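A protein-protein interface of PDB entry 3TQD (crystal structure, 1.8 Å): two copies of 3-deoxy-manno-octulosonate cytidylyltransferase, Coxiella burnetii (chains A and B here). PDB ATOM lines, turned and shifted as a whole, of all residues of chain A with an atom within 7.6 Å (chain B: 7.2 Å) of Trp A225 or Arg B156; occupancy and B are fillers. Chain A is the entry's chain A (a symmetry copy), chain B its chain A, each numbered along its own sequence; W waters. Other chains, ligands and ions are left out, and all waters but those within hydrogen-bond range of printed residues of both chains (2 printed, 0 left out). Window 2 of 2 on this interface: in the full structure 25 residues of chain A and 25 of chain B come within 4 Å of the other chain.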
ATOM      1  N   TRP A 207       5.627  14.174 -22.572  1.00  0.00           N
ATOM      2  CA  TRP A 207       5.863  13.126 -23.559  1.00  0.00           C
ATOM      3  C   TRP A 207       4.598  12.302 -23.748  1.00  0.00           C
ATOM      4  O   TRP A 207       3.938  11.927 -22.777  1.00  0.00           O
ATOM      5  CB  TRP A 207       6.998  12.217 -23.099  1.00  0.00           C
ATOM      6  CG  TRP A 207       8.359  12.840 -23.135  1.00  0.00           C
ATOM      7  CD1 TRP A 207       8.756  13.964 -23.839  1.00  0.00           C
ATOM      8  CD2 TRP A 207       9.511  12.364 -22.455  1.00  0.00           C
ATOM      9  NE1 TRP A 207      10.094  14.211 -23.596  1.00  0.00           N
ATOM     10  CE2 TRP A 207      10.573  13.234 -22.755  1.00  0.00           C
ATOM     11  CE3 TRP A 207       9.756  11.266 -21.613  1.00  0.00           C
ATOM     12  CZ2 TRP A 207      11.865  13.043 -22.231  1.00  0.00           C
ATOM     13  CZ3 TRP A 207      11.029  11.109 -21.070  1.00  0.00           C
ATOM     14  CH2 TRP A 207      12.068  11.972 -21.407  1.00  0.00           C
ATOM     15  N   ASP A 208       4.275  11.976 -24.990  1.00  0.00           N
ATOM     16  CA  ASP A 208       3.187  11.053 -25.202  1.00  0.00           C
ATOM     17  C   ASP A 208       3.640   9.589 -25.129  1.00  0.00           C
ATOM     18  O   ASP A 208       4.850   9.264 -25.194  1.00  0.00           O
ATOM     19  CB  ASP A 208       2.446  11.312 -26.503  1.00  0.00           C
ATOM     20  CG  ASP A 208       0.947  11.182 -26.318  1.00  0.00           C
ATOM     21  OD1 ASP A 208       0.563  10.358 -25.439  1.00  0.00           O
ATOM     22  OD2 ASP A 208       0.167  11.925 -27.002  1.00  0.00           O
ATOM     23  N   ALA A 209       2.643   8.728 -24.941  1.00  0.00           N
ATOM     24  CA  ALA A 209       2.839   7.305 -24.906  1.00  0.00           C
ATOM     25  C   ALA A 209       3.340   6.776 -26.239  1.00  0.00           C
ATOM     26  O   ALA A 209       3.237   7.429 -27.320  1.00  0.00           O
ATOM     27  CB  ALA A 209       1.543   6.607 -24.504  1.00  0.00           C
ATOM     28  N   CYS A 210       3.871   5.575 -26.181  1.00  0.00           N
ATOM     29  CA  CYS A 210       4.354   4.901 -27.348  1.00  0.00           C
ATOM     30  C   CYS A 210       3.713   3.522 -27.467  1.00  0.00           C
ATOM     31  O   CYS A 210       3.200   3.005 -26.487  1.00  0.00           O
ATOM     32  CB  CYS A 210       5.861   4.794 -27.305  1.00  0.00           C
ATOM     33  SG  CYS A 210       6.542   3.866 -25.984  1.00  0.00           S
ATOM     34  N   PRO A 211       3.714   2.954 -28.685  1.00  0.00           N
ATOM     35  CA  PRO A 211       3.092   1.645 -28.874  1.00  0.00           C
ATOM     36  C   PRO A 211       3.658   0.589 -27.935  1.00  0.00           C
ATOM     37  O   PRO A 211       2.891  -0.211 -27.411  1.00  0.00           O
ATOM     38  CB  PRO A 211       3.417   1.287 -30.341  1.00  0.00           C
ATOM     39  CG  PRO A 211       4.003   2.539 -30.959  1.00  0.00           C
ATOM     40  CD  PRO A 211       3.832   3.655 -29.971  1.00  0.00           C
ATOM     41  N   ALA A 212       4.969   0.590 -27.713  1.00  0.00           N
ATOM     42  CA  ALA A 212       5.584  -0.494 -26.941  1.00  0.00           C
ATOM     43  C   ALA A 212       5.146  -0.466 -25.469  1.00  0.00           C
ATOM     44  O   ALA A 212       4.839  -1.494 -24.891  1.00  0.00           O
ATOM     45  CB  ALA A 212       7.090  -0.480 -27.077  1.00  0.00           C
ATOM     46  N   GLU A 213       5.082   0.732 -24.892  1.00  0.00           N
ATOM     47  CA  GLU A 213       4.602   0.910 -23.528  1.00  0.00           C
ATOM     48  C   GLU A 213       3.152   0.379 -23.401  1.00  0.00           C
ATOM     49  O   GLU A 213       2.794  -0.222 -22.367  1.00  0.00           O
ATOM     50  CB  GLU A 213       4.694   2.417 -23.205  1.00  0.00           C
ATOM     51  CG  GLU A 213       3.851   2.899 -22.111  1.00  0.00           C
ATOM     52  CD  GLU A 213       3.666   4.394 -22.130  1.00  0.00           C
ATOM     53  OE1 GLU A 213       4.167   5.111 -23.041  1.00  0.00           O
ATOM     54  OE2 GLU A 213       2.955   4.845 -21.221  1.00  0.00           O
ATOM     55  N   GLN A 220       7.389   2.879 -18.122  1.00  0.00           N
ATOM     56  CA  GLN A 220       8.838   3.247 -18.187  1.00  0.00           C
ATOM     57  C   GLN A 220       9.408   3.210 -19.608  1.00  0.00           C
ATOM     58  O   GLN A 220      10.401   3.888 -19.863  1.00  0.00           O
ATOM     59  CB  GLN A 220       9.655   2.437 -17.241  1.00  0.00           C
ATOM     60  CG  GLN A 220       9.782   0.954 -17.488  1.00  0.00           C
ATOM     61  CD  GLN A 220       8.725   0.100 -16.801  1.00  0.00           C
ATOM     62  OE1 GLN A 220       7.523   0.445 -16.753  1.00  0.00           O
ATOM     63  NE2 GLN A 220       9.155  -1.016 -16.298  1.00  0.00           N
ATOM     64  N   LEU A 221       8.792   2.431 -20.500  1.00  0.00           N
ATOM     65  CA  LEU A 221       9.232   2.396 -21.899  1.00  0.00           C
ATOM     66  C   LEU A 221       9.095   3.740 -22.566  1.00  0.00           C
ATOM     67  O   LEU A 221       9.846   4.048 -23.517  1.00  0.00           O
ATOM     68  CB  LEU A 221       8.540   1.322 -22.683  1.00  0.00           C
ATOM     69  CG  LEU A 221       8.893  -0.088 -22.218  1.00  0.00           C
ATOM     70  CD1 LEU A 221       8.080  -1.105 -23.018  1.00  0.00           C
ATOM     71  CD2 LEU A 221      10.406  -0.318 -22.328  1.00  0.00           C
ATOM     72  N   ARG A 222       8.200   4.582 -22.060  1.00  0.00           N
ATOM     73  CA  ARG A 222       8.076   5.904 -22.570  1.00  0.00           C
ATOM     74  C   ARG A 222       9.383   6.710 -22.518  1.00  0.00           C
ATOM     75  O   ARG A 222       9.667   7.466 -23.432  1.00  0.00           O
ATOM     76  CB  ARG A 222       6.904   6.651 -21.864  1.00  0.00           C
ATOM     77  CG  ARG A 222       6.530   7.935 -22.565  1.00  0.00           C
ATOM     78  CD  ARG A 222       5.420   8.716 -21.807  1.00  0.00           C
ATOM     79  NE  ARG A 222       4.303   7.848 -21.412  1.00  0.00           N
ATOM     80  CZ  ARG A 222       3.234   8.258 -20.708  1.00  0.00           C
ATOM     81  NH1 ARG A 222       3.096   9.518 -20.341  1.00  0.00           N
ATOM     82  NH2 ARG A 222       2.281   7.396 -20.402  1.00  0.00           N
ATOM     83  N   ILE A 223      10.097   6.611 -21.410  1.00  0.00           N
ATOM     84  CA  ILE A 223      11.371   7.294 -21.215  1.00  0.00           C
ATOM     85  C   ILE A 223      12.364   6.831 -22.313  1.00  0.00           C
ATOM     86  O   ILE A 223      13.000   7.654 -22.954  1.00  0.00           O
ATOM     87  CB  ILE A 223      11.948   7.048 -19.807  1.00  0.00           C
ATOM     88  CG1 ILE A 223      11.030   7.592 -18.686  1.00  0.00           C
ATOM     89  CG2 ILE A 223      13.383   7.642 -19.682  1.00  0.00           C
ATOM     90  CD1 ILE A 223      11.302   7.060 -17.286  1.00  0.00           C
ATOM     91  N   LEU A 224      12.525   5.501 -22.450  1.00  0.00           N
ATOM     92  CA  LEU A 224      13.398   4.960 -23.508  1.00  0.00           C
ATOM     93  C   LEU A 224      12.977   5.398 -24.910  1.00  0.00           C
ATOM     94  O   LEU A 224      13.804   5.818 -25.705  1.00  0.00           O
ATOM     95  CB  LEU A 224      13.537   3.419 -23.358  1.00  0.00           C
ATOM     96  CG  LEU A 224      13.940   2.864 -22.012  1.00  0.00           C
ATOM     97  CD1 LEU A 224      14.216   1.327 -22.195  1.00  0.00           C
ATOM     98  CD2 LEU A 224      15.125   3.600 -21.273  1.00  0.00           C
ATOM     99  N   TRP A 225      11.679   5.398 -25.190  1.00  0.00           N
ATOM    100  CA  TRP A 225      11.141   5.763 -26.490  1.00  0.00           C
ATOM    101  C   TRP A 225      11.605   7.169 -26.879  1.00  0.00           C
ATOM    102  O   TRP A 225      11.970   7.427 -28.005  1.00  0.00           O
ATOM    103  CB  TRP A 225       9.591   5.636 -26.509  1.00  0.00           C
ATOM    104  CG  TRP A 225       8.811   6.298 -27.742  1.00  0.00           C
ATOM    105  CD1 TRP A 225       8.083   7.449 -27.737  1.00  0.00           C
ATOM    106  CD2 TRP A 225       8.602   5.707 -29.003  1.00  0.00           C
ATOM    107  NE1 TRP A 225       7.481   7.663 -28.982  1.00  0.00           N
ATOM    108  CE2 TRP A 225       7.787   6.568 -29.760  1.00  0.00           C
ATOM    109  CE3 TRP A 225       9.058   4.512 -29.591  1.00  0.00           C
ATOM    110  CZ2 TRP A 225       7.422   6.274 -31.074  1.00  0.00           C
ATOM    111  CZ3 TRP A 225       8.694   4.233 -30.876  1.00  0.00           C
ATOM    112  CH2 TRP A 225       7.894   5.097 -31.614  1.00  0.00           C
ATOM    113  N   HIS A 226      11.634   8.040 -25.874  1.00  0.00           N
ATOM    114  CA  HIS A 226      11.885   9.465 -26.072  1.00  0.00           C
ATOM    115  C   HIS A 226      13.371   9.791 -25.926  1.00  0.00           C
ATOM    116  O   HIS A 226      13.791  10.957 -25.950  1.00  0.00           O
ATOM    117  CB  HIS A 226      11.028  10.272 -25.113  1.00  0.00           C
ATOM    118  CG  HIS A 226       9.626  10.456 -25.606  1.00  0.00           C
ATOM    119  ND1 HIS A 226       9.310  11.346 -26.607  1.00  0.00           N
ATOM    120  CD2 HIS A 226       8.467   9.838 -25.269  1.00  0.00           C
ATOM    121  CE1 HIS A 226       8.016  11.276 -26.866  1.00  0.00           C
ATOM    122  NE2 HIS A 226       7.478  10.370 -26.068  1.00  0.00           N
ATOM    123  N   GLY A 227      14.203   8.753 -25.894  1.00  0.00           N
ATOM    124  CA  GLY A 227      15.648   8.971 -25.914  1.00  0.00           C
ATOM    125  C   GLY A 227      16.226   9.234 -24.534  1.00  0.00           C
ATOM    126  O   GLY A 227      17.422   9.594 -24.405  1.00  0.00           O
ATOM    127  N   GLY A 228      15.404   9.083 -23.519  1.00  0.00           N
ATOM    128  CA  GLY A 228      15.815   9.237 -22.139  1.00  0.00           C
ATOM    129  C   GLY A 228      16.538   7.988 -21.706  1.00  0.00           C
ATOM    130  O   GLY A 228      16.444   6.951 -22.353  1.00  0.00           O
ATOM    131  N   VAL B 153      13.480  -3.587 -31.442  1.00  0.00           N
ATOM    132  CA  VAL B 153      12.572  -2.576 -30.868  1.00  0.00           C
ATOM    133  C   VAL B 153      13.204  -1.237 -31.062  1.00  0.00           C
ATOM    134  O   VAL B 153      14.423  -1.035 -30.827  1.00  0.00           O
ATOM    135  CB  VAL B 153      12.245  -2.863 -29.415  1.00  0.00           C
ATOM    136  CG1 VAL B 153      11.347  -1.782 -28.843  1.00  0.00           C
ATOM    137  CG2 VAL B 153      11.569  -4.198 -29.273  1.00  0.00           C
ATOM    138  N   LEU B 154      12.369  -0.311 -31.546  1.00  0.00           N
ATOM    139  CA  LEU B 154      12.812   1.018 -31.929  1.00  0.00           C
ATOM    140  C   LEU B 154      12.399   2.115 -30.954  1.00  0.00           C
ATOM    141  O   LEU B 154      11.375   2.050 -30.290  1.00  0.00           O
ATOM    142  CB  LEU B 154      12.246   1.386 -33.304  1.00  0.00           C
ATOM    143  CG  LEU B 154      12.422   0.450 -34.483  1.00  0.00           C
ATOM    144  CD1 LEU B 154      11.735   0.968 -35.801  1.00  0.00           C
ATOM    145  CD2 LEU B 154      13.876   0.163 -34.747  1.00  0.00           C
ATOM    146  N   ASN B 155      13.210   3.151 -30.865  1.00  0.00           N
ATOM    147  CA  ASN B 155      12.747   4.352 -30.202  1.00  0.00           C
ATOM    148  C   ASN B 155      12.119   5.308 -31.208  1.00  0.00           C
ATOM    149  O   ASN B 155      11.958   4.986 -32.384  1.00  0.00           O
ATOM    150  CB  ASN B 155      13.878   5.053 -29.399  1.00  0.00           C
ATOM    151  CG  ASN B 155      14.873   5.822 -30.248  1.00  0.00           C
ATOM    152  OD1 ASN B 155      14.711   6.111 -31.465  1.00  0.00           O
ATOM    153  ND2 ASN B 155      15.915   6.271 -29.555  1.00  0.00           N
ATOM    154  N   ARG B 156      11.716   6.465 -30.700  1.00  0.00           N
ATOM    155  CA  ARG B 156      10.918   7.383 -31.527  1.00  0.00           C
ATOM    156  C   ARG B 156      11.631   7.809 -32.789  1.00  0.00           C
ATOM    157  O   ARG B 156      10.970   8.028 -33.815  1.00  0.00           O
ATOM    158  CB  ARG B 156      10.501   8.597 -30.717  1.00  0.00           C
ATOM    159  CG  ARG B 156       9.399   9.436 -31.414  1.00  0.00           C
ATOM    160  CD  ARG B 156       8.956  10.595 -30.525  1.00  0.00           C
ATOM    161  NE  ARG B 156       9.946  11.678 -30.486  1.00  0.00           N
ATOM    162  CZ  ARG B 156      10.247  12.505 -31.488  1.00  0.00           C
ATOM    163  NH1 ARG B 156       9.612  12.457 -32.664  1.00  0.00           N
ATOM    164  NH2 ARG B 156      11.196  13.418 -31.305  1.00  0.00           N
ATOM    165  N   ARG B 157      12.948   7.948 -32.704  1.00  0.00           N
ATOM    166  CA  ARG B 157      13.765   8.363 -33.826  1.00  0.00           C
ATOM    167  C   ARG B 157      14.396   7.224 -34.609  1.00  0.00           C
ATOM    168  O   ARG B 157      15.320   7.454 -35.401  1.00  0.00           O
ATOM    169  CB  ARG B 157      14.815   9.321 -33.324  1.00  0.00           C
ATOM    170  CG  ARG B 157      14.154  10.638 -32.815  1.00  0.00           C
ATOM    171  CD  ARG B 157      15.069  11.789 -32.876  1.00  0.00           C
ATOM    172  NE  ARG B 157      14.340  13.063 -32.752  1.00  0.00           N
ATOM    173  CZ  ARG B 157      13.821  13.776 -33.767  1.00  0.00           C
ATOM    174  NH1 ARG B 157      13.916  13.371 -35.026  1.00  0.00           N
ATOM    175  NH2 ARG B 157      13.199  14.924 -33.513  1.00  0.00           N
ATOM    176  N   ASN B 158      13.820   6.030 -34.441  1.00  0.00           N
ATOM    177  CA  ASN B 158      14.209   4.826 -35.084  1.00  0.00           C
ATOM    178  C   ASN B 158      15.606   4.311 -34.707  1.00  0.00           C
ATOM    179  O   ASN B 158      16.163   3.517 -35.475  1.00  0.00           O
ATOM    180  CB  ASN B 158      14.068   4.871 -36.636  1.00  0.00           C
ATOM    181  CG  ASN B 158      12.670   4.674 -37.113  1.00  0.00           C
ATOM    182  OD1 ASN B 158      12.414   4.719 -38.336  1.00  0.00           O
ATOM    183  ND2 ASN B 158      11.743   4.558 -36.202  1.00  0.00           N
ATOM    184  N   TYR B 159      16.129   4.685 -33.530  1.00  0.00           N
ATOM    185  CA  TYR B 159      17.362   4.007 -32.983  1.00  0.00           C
ATOM    186  C   TYR B 159      16.977   2.678 -32.350  1.00  0.00           C
ATOM    187  O   TYR B 159      15.839   2.536 -31.825  1.00  0.00           O
ATOM    188  CB  TYR B 159      18.055   4.865 -31.976  1.00  0.00           C
ATOM    189  CG  TYR B 159      18.725   6.013 -32.609  1.00  0.00           C
ATOM    190  CD1 TYR B 159      18.061   7.257 -32.708  1.00  0.00           C
ATOM    191  CD2 TYR B 159      20.008   5.903 -33.178  1.00  0.00           C
ATOM    192  CE1 TYR B 159      18.635   8.312 -33.337  1.00  0.00           C
ATOM    193  CE2 TYR B 159      20.608   7.020 -33.766  1.00  0.00           C
ATOM    194  CZ  TYR B 159      19.898   8.203 -33.859  1.00  0.00           C
ATOM    195  OH  TYR B 159      20.420   9.323 -34.435  1.00  0.00           O
ATOM    196  N   LEU B 161      16.632   0.021 -29.589  1.00  0.00           N
ATOM    197  CA  LEU B 161      16.764  -0.111 -28.150  1.00  0.00           C
ATOM    198  C   LEU B 161      17.328  -1.436 -27.763  1.00  0.00           C
ATOM    199  O   LEU B 161      18.069  -1.523 -26.766  1.00  0.00           O
ATOM    200  CB  LEU B 161      15.401   0.061 -27.460  1.00  0.00           C
ATOM    201  CG  LEU B 161      14.769   1.494 -27.531  1.00  0.00           C
ATOM    202  CD1 LEU B 161      13.327   1.415 -26.931  1.00  0.00           C
ATOM    203  CD2 LEU B 161      15.660   2.468 -26.803  1.00  0.00           C
HETATM  204  O   HOH W   1      16.606   5.800 -26.602  1.00  0.00           O
HETATM  205  O   HOH W   2      13.820   9.161 -29.601  1.00  0.00           O
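The backbone NH (N) of Leu B161 lies within hydrogen-bond range of the backbone carbonyl oxygen (O) of Val B153, at 2.7 Å.
The side-chain amide oxygen (OD1) of Asn B155 sits at hydrogen-bond distance from the backbone NH (N) of Arg B157, 2.8 Å away.
OD1 of Asn B155 is in hydrogen-bond range of N of Asn B158, 3.1 Å away.
The side-chain amide oxygen (OD1) of Asn B155 lies within hydrogen-bond range of the backbone NH (N) of Tyr B159 (2.9 Å).
O of Asp A208 is in hydrogen-bond range of NE2 of His A226 (3.0 Å).
Water W1 bridges the backbone carbonyl oxygen (O) of Leu A224 and the side-chain amide nitrogen (ND2) of Asn B155.
Water W2 bridges O of Trp A225 and N of Arg B157.
Of the printed residues of chain B, Trp A225 touches Leu B154 (3.5 Å), Asn B155 (3.3 Å) and Arg B156 (2.9 Å).
Arg B156 touches just these residues of chain A: Trp A225 (2.9 Å) and His A226 (3.8 Å).
Printed residues of chain B within 4 Å of His A226: Arg B156.
Of the printed residues of chain A, Leu B161 touches Leu A224.
Printed residues of chain A within 4 Å of Asn B155: Leu A224 (3.8 Å) and Trp A225 (3.3 Å).
Arg A222 touches none of the printed residues of chain B.
The nearest printed residue of chain B that does not touch His A226 is Asn B155 (5.1 Å).
No position is printed for both chains.
Of the 6 pairs that touch across the chains among the printed residues, none has its exchanged pair printed and touching as well.
Among the printed residues, merely in contact across the chains: Trp A225 with Asn B155 (3.3 Å), Trp A225 with Leu B154 (3.5 Å), Leu A224 with Asn B155 (3.8 Å), His A226 with Arg B156 (3.8 Å) and Leu A224 with Leu B161 (3.98 Å).
Of the 8 printed residues of chain B, 4 touch a printed residue of chain A.
Hydrophobic or aromatic side chains of chain B that line the printed part of chain A: Leu B161.
Of the 16 printed residues of chain A, 3 touch a printed residue of chain B.
Among the printed residues, 6 pairs touch across the chains.
The backbone carbonyl oxygen of Trp A225 lies within hydrogen-bond range of the backbone NH of Arg B156.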
